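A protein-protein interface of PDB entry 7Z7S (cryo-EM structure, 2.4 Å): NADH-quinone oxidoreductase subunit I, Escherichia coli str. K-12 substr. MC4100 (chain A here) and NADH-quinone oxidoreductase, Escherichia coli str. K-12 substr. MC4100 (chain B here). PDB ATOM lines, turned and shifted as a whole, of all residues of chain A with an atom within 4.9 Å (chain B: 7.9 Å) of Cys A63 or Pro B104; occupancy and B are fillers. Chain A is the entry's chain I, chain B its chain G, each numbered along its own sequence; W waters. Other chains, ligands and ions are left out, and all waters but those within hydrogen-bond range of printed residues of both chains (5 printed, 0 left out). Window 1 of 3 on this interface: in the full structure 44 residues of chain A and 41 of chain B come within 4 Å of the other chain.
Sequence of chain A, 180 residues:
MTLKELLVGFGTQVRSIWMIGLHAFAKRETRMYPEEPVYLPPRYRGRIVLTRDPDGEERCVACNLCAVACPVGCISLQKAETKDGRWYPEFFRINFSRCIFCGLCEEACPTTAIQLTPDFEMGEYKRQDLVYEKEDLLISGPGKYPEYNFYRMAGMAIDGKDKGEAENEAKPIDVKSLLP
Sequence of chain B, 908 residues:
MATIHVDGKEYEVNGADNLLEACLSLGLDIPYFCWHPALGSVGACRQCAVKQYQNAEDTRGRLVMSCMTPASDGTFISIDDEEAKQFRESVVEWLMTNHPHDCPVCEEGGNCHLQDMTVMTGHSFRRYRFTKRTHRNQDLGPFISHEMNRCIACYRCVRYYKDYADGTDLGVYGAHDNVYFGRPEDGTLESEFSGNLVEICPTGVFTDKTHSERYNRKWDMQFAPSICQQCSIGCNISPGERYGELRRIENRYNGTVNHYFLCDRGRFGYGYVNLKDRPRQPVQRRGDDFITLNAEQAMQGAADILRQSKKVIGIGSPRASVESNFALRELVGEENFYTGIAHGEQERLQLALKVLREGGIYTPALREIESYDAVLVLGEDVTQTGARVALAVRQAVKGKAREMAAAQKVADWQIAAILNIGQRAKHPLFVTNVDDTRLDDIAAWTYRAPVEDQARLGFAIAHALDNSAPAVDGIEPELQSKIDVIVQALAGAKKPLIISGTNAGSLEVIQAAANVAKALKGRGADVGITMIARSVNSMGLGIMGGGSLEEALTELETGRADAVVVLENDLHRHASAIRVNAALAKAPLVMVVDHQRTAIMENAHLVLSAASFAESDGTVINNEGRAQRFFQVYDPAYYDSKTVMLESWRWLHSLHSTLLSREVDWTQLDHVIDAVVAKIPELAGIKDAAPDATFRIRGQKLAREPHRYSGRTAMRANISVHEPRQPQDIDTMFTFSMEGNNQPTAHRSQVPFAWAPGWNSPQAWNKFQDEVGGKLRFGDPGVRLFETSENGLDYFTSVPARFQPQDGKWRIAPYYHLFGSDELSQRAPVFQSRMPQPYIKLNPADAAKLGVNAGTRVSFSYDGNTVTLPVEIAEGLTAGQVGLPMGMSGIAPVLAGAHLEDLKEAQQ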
ATOM      1  N   VAL A  61       1.709 -18.996   8.014  1.00  0.00           N
ATOM      2  CA  VAL A  61       2.571 -20.096   7.630  1.00  0.00           C
ATOM      3  C   VAL A  61       2.160 -21.390   8.314  1.00  0.00           C
ATOM      4  O   VAL A  61       2.910 -22.363   8.283  1.00  0.00           O
ATOM      5  CB  VAL A  61       4.040 -19.761   7.917  1.00  0.00           C
ATOM      6  CG1 VAL A  61       4.454 -18.527   7.158  1.00  0.00           C
ATOM      7  CG2 VAL A  61       4.268 -19.574   9.407  1.00  0.00           C
ATOM      8  N   ALA A  62       0.985 -21.405   8.947  1.00  0.00           N
ATOM      9  CA  ALA A  62       0.415 -22.579   9.609  1.00  0.00           C
ATOM     10  C   ALA A  62       1.371 -23.171  10.640  1.00  0.00           C
ATOM     11  O   ALA A  62       1.522 -24.385  10.757  1.00  0.00           O
ATOM     12  CB  ALA A  62      -0.017 -23.629   8.592  1.00  0.00           C
ATOM     13  N   CYS A  63       2.026 -22.295  11.389  1.00  0.00           N
ATOM     14  CA  CYS A  63       3.001 -22.697  12.385  1.00  0.00           C
ATOM     15  C   CYS A  63       2.370 -23.224  13.665  1.00  0.00           C
ATOM     16  O   CYS A  63       3.087 -23.804  14.486  1.00  0.00           O
ATOM     17  CB  CYS A  63       3.909 -21.513  12.699  1.00  0.00           C
ATOM     18  SG  CYS A  63       3.238 -20.320  13.840  1.00  0.00           S
ATOM     19  N   ASN A  64       1.065 -23.015  13.847  1.00  0.00           N
ATOM     20  CA  ASN A  64       0.250 -23.522  14.950  1.00  0.00           C
ATOM     21  C   ASN A  64       0.604 -22.926  16.305  1.00  0.00           C
ATOM     22  O   ASN A  64       0.230 -23.488  17.332  1.00  0.00           O
ATOM     23  CB  ASN A  64       0.295 -25.052  15.038  1.00  0.00           C
ATOM     24  CG  ASN A  64      -0.993 -25.690  14.616  1.00  0.00           C
ATOM     25  OD1 ASN A  64      -1.997 -25.588  15.304  1.00  0.00           O
ATOM     26  ND2 ASN A  64      -0.975 -26.351  13.475  1.00  0.00           N
ATOM     27  N   LEU A  65       1.295 -21.788  16.350  1.00  0.00           N
ATOM     28  CA  LEU A  65       1.581 -21.170  17.640  1.00  0.00           C
ATOM     29  C   LEU A  65       0.341 -20.522  18.248  1.00  0.00           C
ATOM     30  O   LEU A  65       0.180 -20.530  19.471  1.00  0.00           O
ATOM     31  CB  LEU A  65       2.702 -20.143  17.497  1.00  0.00           C
ATOM     32  CG  LEU A  65       4.141 -20.662  17.468  1.00  0.00           C
ATOM     33  CD1 LEU A  65       5.114 -19.508  17.493  1.00  0.00           C
ATOM     34  CD2 LEU A  65       4.428 -21.625  18.608  1.00  0.00           C
ATOM     35  N   LEU A  77      -6.229 -25.670  12.885  1.00  0.00           N
ATOM     36  CA  LEU A  77      -5.691 -25.456  11.550  1.00  0.00           C
ATOM     37  C   LEU A  77      -4.805 -26.637  11.175  1.00  0.00           C
ATOM     38  O   LEU A  77      -4.492 -27.485  12.007  1.00  0.00           O
ATOM     39  CB  LEU A  77      -4.918 -24.137  11.475  1.00  0.00           C
ATOM     40  CG  LEU A  77      -3.678 -24.069  12.360  1.00  0.00           C
ATOM     41  CD1 LEU A  77      -2.451 -23.851  11.518  1.00  0.00           C
ATOM     42  CD2 LEU A  77      -3.805 -22.991  13.408  1.00  0.00           C
ATOM     43  N   TRP A  87       4.737 -22.532   3.331  1.00  0.00           N
ATOM     44  CA  TRP A  87       3.759 -23.110   4.236  1.00  0.00           C
ATOM     45  C   TRP A  87       2.534 -22.211   4.306  1.00  0.00           C
ATOM     46  O   TRP A  87       2.654 -20.985   4.305  1.00  0.00           O
ATOM     47  CB  TRP A  87       4.350 -23.269   5.635  1.00  0.00           C
ATOM     48  CG  TRP A  87       5.376 -24.335   5.831  1.00  0.00           C
ATOM     49  CD1 TRP A  87       6.220 -24.848   4.901  1.00  0.00           C
ATOM     50  CD2 TRP A  87       5.683 -24.999   7.061  1.00  0.00           C
ATOM     51  NE1 TRP A  87       7.031 -25.793   5.469  1.00  0.00           N
ATOM     52  CE2 TRP A  87       6.719 -25.906   6.795  1.00  0.00           C
ATOM     53  CE3 TRP A  87       5.175 -24.915   8.359  1.00  0.00           C
ATOM     54  CZ2 TRP A  87       7.256 -26.728   7.778  1.00  0.00           C
ATOM     55  CZ3 TRP A  87       5.709 -25.729   9.330  1.00  0.00           C
ATOM     56  CH2 TRP A  87       6.740 -26.624   9.037  1.00  0.00           C
ATOM     57  N   PRO A 110       4.026 -15.178  15.015  1.00  0.00           N
ATOM     58  CA  PRO A 110       5.323 -14.665  14.570  1.00  0.00           C
ATOM     59  C   PRO A 110       5.335 -14.098  13.159  1.00  0.00           C
ATOM     60  O   PRO A 110       6.402 -13.713  12.680  1.00  0.00           O
ATOM     61  CB  PRO A 110       6.204 -15.915  14.654  1.00  0.00           C
ATOM     62  CG  PRO A 110       5.274 -17.031  14.376  1.00  0.00           C
ATOM     63  CD  PRO A 110       3.891 -16.622  14.767  1.00  0.00           C
ATOM     64  N   PHE A 150       7.061 -12.099   6.973  1.00  0.00           N
ATOM     65  CA  PHE A 150       7.861 -13.111   7.651  1.00  0.00           C
ATOM     66  C   PHE A 150       8.825 -13.783   6.689  1.00  0.00           C
ATOM     67  O   PHE A 150       9.968 -14.079   7.052  1.00  0.00           O
ATOM     68  CB  PHE A 150       6.967 -14.165   8.304  1.00  0.00           C
ATOM     69  CG  PHE A 150       7.694 -15.432   8.660  1.00  0.00           C
ATOM     70  CD1 PHE A 150       8.534 -15.470   9.755  1.00  0.00           C
ATOM     71  CD2 PHE A 150       7.557 -16.577   7.890  1.00  0.00           C
ATOM     72  CE1 PHE A 150       9.215 -16.618  10.082  1.00  0.00           C
ATOM     73  CE2 PHE A 150       8.242 -17.720   8.211  1.00  0.00           C
ATOM     74  CZ  PHE A 150       9.069 -17.743   9.312  1.00  0.00           C
ATOM     75  N   PRO B 100      19.053 -19.617  10.721  1.00  0.00           N
ATOM     76  CA  PRO B 100      17.984 -18.935   9.989  1.00  0.00           C
ATOM     77  C   PRO B 100      16.764 -18.679  10.855  1.00  0.00           C
ATOM     78  O   PRO B 100      16.497 -19.388  11.824  1.00  0.00           O
ATOM     79  CB  PRO B 100      17.660 -19.911   8.858  1.00  0.00           C
ATOM     80  CG  PRO B 100      17.978 -21.224   9.421  1.00  0.00           C
ATOM     81  CD  PRO B 100      19.144 -21.033  10.345  1.00  0.00           C
ATOM     82  N   HIS B 101      16.005 -17.657  10.466  1.00  0.00           N
ATOM     83  CA  HIS B 101      14.795 -17.228  11.163  1.00  0.00           C
ATOM     84  C   HIS B 101      13.628 -18.129  10.746  1.00  0.00           C
ATOM     85  O   HIS B 101      12.661 -17.708  10.112  1.00  0.00           O
ATOM     86  CB  HIS B 101      14.529 -15.764  10.841  1.00  0.00           C
ATOM     87  CG  HIS B 101      13.607 -15.076  11.797  1.00  0.00           C
ATOM     88  ND1 HIS B 101      14.056 -14.407  12.913  1.00  0.00           N
ATOM     89  CD2 HIS B 101      12.263 -14.928  11.786  1.00  0.00           C
ATOM     90  CE1 HIS B 101      13.027 -13.891  13.558  1.00  0.00           C
ATOM     91  NE2 HIS B 101      11.928 -14.191  12.893  1.00  0.00           N
ATOM     92  N   ASP B 102      13.728 -19.400  11.126  1.00  0.00           N
ATOM     93  CA  ASP B 102      12.961 -20.440  10.464  1.00  0.00           C
ATOM     94  C   ASP B 102      11.962 -21.188  11.335  1.00  0.00           C
ATOM     95  O   ASP B 102      11.211 -21.990  10.781  1.00  0.00           O
ATOM     96  CB  ASP B 102      13.902 -21.480   9.839  1.00  0.00           C
ATOM     97  CG  ASP B 102      14.190 -21.220   8.395  1.00  0.00           C
ATOM     98  OD1 ASP B 102      13.928 -20.104   7.918  1.00  0.00           O
ATOM     99  OD2 ASP B 102      14.696 -22.142   7.735  1.00  0.00           O
ATOM    100  N   CYS B 103      11.930 -20.958  12.649  1.00  0.00           N
ATOM    101  CA  CYS B 103      11.129 -21.778  13.564  1.00  0.00           C
ATOM    102  C   CYS B 103       9.654 -21.940  13.187  1.00  0.00           C
ATOM    103  O   CYS B 103       9.149 -23.066  13.316  1.00  0.00           O
ATOM    104  CB  CYS B 103      11.218 -21.231  14.999  1.00  0.00           C
ATOM    105  SG  CYS B 103      12.818 -21.235  15.792  1.00  0.00           S
ATOM    106  N   PRO B 104       8.913 -20.912  12.734  1.00  0.00           N
ATOM    107  CA  PRO B 104       7.532 -21.167  12.291  1.00  0.00           C
ATOM    108  C   PRO B 104       7.402 -22.129  11.121  1.00  0.00           C
ATOM    109  O   PRO B 104       6.406 -22.852  11.045  1.00  0.00           O
ATOM    110  CB  PRO B 104       7.026 -19.768  11.922  1.00  0.00           C
ATOM    111  CG  PRO B 104       7.839 -18.871  12.706  1.00  0.00           C
ATOM    112  CD  PRO B 104       9.178 -19.459  12.739  1.00  0.00           C
ATOM    113  N   VAL B 105       8.370 -22.175  10.212  1.00  0.00           N
ATOM    114  CA  VAL B 105       8.259 -23.045   9.046  1.00  0.00           C
ATOM    115  C   VAL B 105       9.272 -24.174   9.127  1.00  0.00           C
ATOM    116  O   VAL B 105       9.720 -24.696   8.106  1.00  0.00           O
ATOM    117  CB  VAL B 105       8.438 -22.254   7.741  1.00  0.00           C
ATOM    118  CG1 VAL B 105       7.219 -21.443   7.474  1.00  0.00           C
ATOM    119  CG2 VAL B 105       9.671 -21.378   7.810  1.00  0.00           C
ATOM    120  N   CYS B 106       9.648 -24.552  10.335  1.00  0.00           N
ATOM    121  CA  CYS B 106      10.604 -25.622  10.550  1.00  0.00           C
ATOM    122  C   CYS B 106       9.902 -26.770  11.246  1.00  0.00           C
ATOM    123  O   CYS B 106       9.211 -26.563  12.244  1.00  0.00           O
ATOM    124  CB  CYS B 106      11.783 -25.125  11.375  1.00  0.00           C
ATOM    125  SG  CYS B 106      13.057 -26.311  11.730  1.00  0.00           S
ATOM    126  N   GLU B 107      10.083 -27.980  10.721  1.00  0.00           N
ATOM    127  CA  GLU B 107       9.425 -29.146  11.291  1.00  0.00           C
ATOM    128  C   GLU B 107       9.987 -29.540  12.647  1.00  0.00           C
ATOM    129  O   GLU B 107       9.363 -30.340  13.344  1.00  0.00           O
ATOM    130  CB  GLU B 107       9.528 -30.326  10.333  1.00  0.00           C
ATOM    131  CG  GLU B 107       8.631 -30.207   9.129  1.00  0.00           C
ATOM    132  CD  GLU B 107       9.330 -29.582   7.950  1.00  0.00           C
ATOM    133  OE1 GLU B 107      10.509 -29.195   8.087  1.00  0.00           O
ATOM    134  OE2 GLU B 107       8.703 -29.479   6.882  1.00  0.00           O
ATOM    135  N   GLY B 109      10.430 -27.409  15.197  1.00  0.00           N
ATOM    136  CA  GLY B 109       9.922 -26.503  16.216  1.00  0.00           C
ATOM    137  C   GLY B 109       8.978 -27.115  17.224  1.00  0.00           C
ATOM    138  O   GLY B 109       8.018 -27.787  16.854  1.00  0.00           O
ATOM    139  N   GLN B 115      16.392 -25.266  20.130  1.00  0.00           N
ATOM    140  CA  GLN B 115      15.469 -24.346  20.796  1.00  0.00           C
ATOM    141  C   GLN B 115      15.540 -24.504  22.308  1.00  0.00           C
ATOM    142  O   GLN B 115      15.621 -23.516  23.052  1.00  0.00           O
ATOM    143  CB  GLN B 115      14.036 -24.598  20.325  1.00  0.00           C
ATOM    144  CG  GLN B 115      13.637 -24.008  18.994  1.00  0.00           C
ATOM    145  CD  GLN B 115      12.139 -24.114  18.765  1.00  0.00           C
ATOM    146  OE1 GLN B 115      11.482 -24.979  19.331  1.00  0.00           O
ATOM    147  NE2 GLN B 115      11.597 -23.231  17.946  1.00  0.00           N
ATOM    148  N   ARG B 150      20.021 -24.679   8.903  1.00  0.00           N
ATOM    149  CA  ARG B 150      19.794 -24.861  10.324  1.00  0.00           C
ATOM    150  C   ARG B 150      20.906 -25.626  11.026  1.00  0.00           C
ATOM    151  O   ARG B 150      20.792 -25.873  12.226  1.00  0.00           O
ATOM    152  CB  ARG B 150      18.463 -25.574  10.540  1.00  0.00           C
ATOM    153  CG  ARG B 150      17.288 -24.831   9.973  1.00  0.00           C
ATOM    154  CD  ARG B 150      16.127 -25.739   9.750  1.00  0.00           C
ATOM    155  NE  ARG B 150      15.080 -25.084   8.984  1.00  0.00           N
ATOM    156  CZ  ARG B 150      14.085 -25.723   8.390  1.00  0.00           C
ATOM    157  NH1 ARG B 150      13.969 -27.036   8.463  1.00  0.00           N
ATOM    158  NH2 ARG B 150      13.188 -25.026   7.703  1.00  0.00           N
ATOM    159  N   TYR B 215       2.024 -32.153   8.393  1.00  0.00           N
ATOM    160  CA  TYR B 215       2.803 -31.802   9.568  1.00  0.00           C
ATOM    161  C   TYR B 215       1.901 -31.293  10.679  1.00  0.00           C
ATOM    162  O   TYR B 215       0.926 -30.583  10.433  1.00  0.00           O
ATOM    163  CB  TYR B 215       3.867 -30.748   9.248  1.00  0.00           C
ATOM    164  CG  TYR B 215       4.684 -30.364  10.461  1.00  0.00           C
ATOM    165  CD1 TYR B 215       5.642 -31.225  10.968  1.00  0.00           C
ATOM    166  CD2 TYR B 215       4.466 -29.164  11.124  1.00  0.00           C
ATOM    167  CE1 TYR B 215       6.369 -30.899  12.077  1.00  0.00           C
ATOM    168  CE2 TYR B 215       5.193 -28.829  12.241  1.00  0.00           C
ATOM    169  CZ  TYR B 215       6.145 -29.702  12.711  1.00  0.00           C
ATOM    170  OH  TYR B 215       6.881 -29.386  13.821  1.00  0.00           O
ATOM    171  N   ASN B 216       2.232 -31.679  11.902  1.00  0.00           N
ATOM    172  CA  ASN B 216       1.683 -31.060  13.091  1.00  0.00           C
ATOM    173  C   ASN B 216       2.785 -31.003  14.132  1.00  0.00           C
ATOM    174  O   ASN B 216       3.768 -31.737  14.063  1.00  0.00           O
ATOM    175  CB  ASN B 216       0.464 -31.818  13.626  1.00  0.00           C
ATOM    176  CG  ASN B 216       0.811 -33.203  14.107  1.00  0.00           C
ATOM    177  OD1 ASN B 216       1.103 -34.089  13.314  1.00  0.00           O
ATOM    178  ND2 ASN B 216       0.790 -33.396  15.414  1.00  0.00           N
ATOM    179  N   ARG B 217       2.619 -30.110  15.092  1.00  0.00           N
ATOM    180  CA  ARG B 217       3.603 -29.957  16.142  1.00  0.00           C
ATOM    181  C   ARG B 217       3.451 -31.056  17.187  1.00  0.00           C
ATOM    182  O   ARG B 217       2.418 -31.720  17.278  1.00  0.00           O
ATOM    183  CB  ARG B 217       3.472 -28.581  16.775  1.00  0.00           C
ATOM    184  CG  ARG B 217       3.578 -27.461  15.770  1.00  0.00           C
ATOM    185  CD  ARG B 217       4.998 -26.984  15.660  1.00  0.00           C
ATOM    186  NE  ARG B 217       5.131 -25.870  14.737  1.00  0.00           N
ATOM    187  CZ  ARG B 217       6.223 -25.607  14.037  1.00  0.00           C
ATOM    188  NH1 ARG B 217       7.298 -26.365  14.129  1.00  0.00           N
ATOM    189  NH2 ARG B 217       6.235 -24.559  13.225  1.00  0.00           N
ATOM    190  N   TRP B 219       3.205 -30.957  20.456  1.00  0.00           N
ATOM    191  CA  TRP B 219       2.202 -30.771  21.500  1.00  0.00           C
ATOM    192  C   TRP B 219       0.802 -31.134  21.017  1.00  0.00           C
ATOM    193  O   TRP B 219      -0.049 -31.500  21.826  1.00  0.00           O
ATOM    194  CB  TRP B 219       2.225 -29.335  22.021  1.00  0.00           C
ATOM    195  CG  TRP B 219       2.055 -28.284  20.973  1.00  0.00           C
ATOM    196  CD1 TRP B 219       0.896 -27.919  20.355  1.00  0.00           C
ATOM    197  CD2 TRP B 219       3.077 -27.457  20.422  1.00  0.00           C
ATOM    198  NE1 TRP B 219       1.138 -26.930  19.449  1.00  0.00           N
ATOM    199  CE2 TRP B 219       2.468 -26.617  19.476  1.00  0.00           C
ATOM    200  CE3 TRP B 219       4.452 -27.346  20.633  1.00  0.00           C
ATOM    201  CZ2 TRP B 219       3.180 -25.676  18.748  1.00  0.00           C
ATOM    202  CZ3 TRP B 219       5.157 -26.420  19.904  1.00  0.00           C
ATOM    203  CH2 TRP B 219       4.521 -25.597  18.973  1.00  0.00           C
ATOM    204  N   ASP B 220       0.555 -31.061  19.714  1.00  0.00           N
ATOM    205  CA  ASP B 220      -0.747 -31.379  19.145  1.00  0.00           C
ATOM    206  C   ASP B 220      -0.930 -32.861  18.864  1.00  0.00           C
ATOM    207  O   ASP B 220      -1.978 -33.253  18.352  1.00  0.00           O
ATOM    208  CB  ASP B 220      -0.960 -30.598  17.850  1.00  0.00           C
ATOM    209  CG  ASP B 220      -1.612 -29.264  18.083  1.00  0.00           C
ATOM    210  OD1 ASP B 220      -2.115 -29.038  19.196  1.00  0.00           O
ATOM    211  OD2 ASP B 220      -1.626 -28.440  17.153  1.00  0.00           O
HETATM  212  O   HOH W   1       8.980 -28.228   4.845  1.00  0.00           O
HETATM  213  O   HOH W   2       9.191 -13.750  12.885  1.00  0.00           O
HETATM  214  O   HOH W   3       0.220 -28.685  15.254  1.00  0.00           O
HETATM  215  O   HOH W   4      -0.229 -28.559  11.171  1.00  0.00           O
HETATM  216  O   HOH W   5      -1.015 -26.012  18.155  1.00  0.00           O
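The side-chain carboxylate of Asp B220 lies close to the side-chain amide oxygen of Asn A64.
The backbone carbonyl oxygen (O) of Cys A63 sits at hydrogen-bond distance from the guanidinium group (NE) of Arg B217 (2.9 Å).
SG of Cys A63 lies close to N of Leu A65 (3.5 Å).
NH2 of Arg B217 is in hydrogen-bond range of O of Cys B103 (3.3 Å).
O of Pro B104 is in hydrogen-bond range of NH2 of Arg B217, 2.8 Å away.
The side-chain sulfur (SG) of Cys B106 sits close to the guanidinium group (NH1) of Arg B150, at 3.5 Å.
The backbone carbonyl oxygen (O) of Glu B107 is in hydrogen-bond range of the side-chain hydroxyl (OH) of Tyr B215 (2.7 Å).
NH1 of Arg B217 lies within hydrogen-bond range of O of Gly B109, at 3.2 Å.
Among the printed residues, pairs that only touch across the chains: Trp A87 with Val B105, Trp A87 with Glu B107, Cys A63 with Pro B104, Trp A87 with Pro B104, Pro A110 with Pro B104, Phe A150 with His B101, Val A61 with Val B105, Phe A150 with Pro B104, Val A61 with Pro B104, Trp A87 with Cys B106, Phe A150 with Val B105, Asn A64 with Trp B219, Leu A65 with Trp B219 and Trp A87 with Tyr B215.
Printed residues of chain B within 4 Å of Cys A63: Pro B104 and Arg B217.
Of chain A, only Val A61 (3.7 Å), Cys A63 (3.3 Å), Trp A87 (3.4 Å), Pro A110 (3.6 Å) and Phe A150 (3.7 Å) come within 4 Å of Pro B104.
Printed residues of chain A within 4 Å of Arg B217: Cys A63 (2.9 Å).
Printed residues of chain B within 4 Å of Pro A110: Pro B104.
Of the printed residues of chain A, Cys B106 touches Trp A87.
Printed residues of chain A within 4 Å of Trp B219: Asn A64 (3.9 Å) and Leu A65 (3.99 Å).
The nearest residue of chain B that does not touch Cys A63 is Trp B219 (4.7 Å).
The nearest printed residue of chain A that does not touch Val B105 is Cys A63 (5.2 Å).
Printed residues of chain B that touch a printed residue of chain A: His B101, Pro B104, Val B105, Cys B106, Glu B107, Tyr B215, Arg B217, Trp B219 and Asp B220.
Hydrophobic or aromatic side chains of chain B that line the printed part of chain A: His B101, Pro B104, Val B105, Tyr B215 and Trp B219.
Of the 9 printed residues of chain A, 7 touch a printed residue of chain B.
Printed residues of chain A that touch a printed residue of chain B: Val A61, Cys A63, Asn A64, Leu A65, Trp A87, Pro A110 and Phe A150.
Hydrophobic or aromatic side chains of chain A that line the printed part of chain B: Val A61, Leu A65, Trp A87, Pro A110 and Phe A150.
Among the printed residues, 16 pairs touch across the chains.
Among the printed residues, no Asp or Glu carboxylate lies within 4 Å of a Lys or Arg side-chain nitrogen of the other chain.
Water W1 lies within hydrogen-bond range of the side-chain carboxylate of Glu B107 and the indole nitrogen of Trp A87.
Water W4 lies within hydrogen-bond range of O of Tyr B215 (2.4 Å) and ND2 of Asn A64 (3.3 Å).
Water W3 lies within hydrogen-bond range of OD2 of Asp B220 (2.7 Å), N of Arg B217 (2.8 Å) and ND2 of Asn A64 (3.2 Å).
Water W5 lies within hydrogen-bond range of NE1 of Trp B219 (2.7 Å), OD2 of Asp B220 (2.7 Å) and O of Asn A64 (2.9 Å).
Water W2 lies within hydrogen-bond range of NE2 of His B101 (2.8 Å) and O of Pro A110 (2.8 Å).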
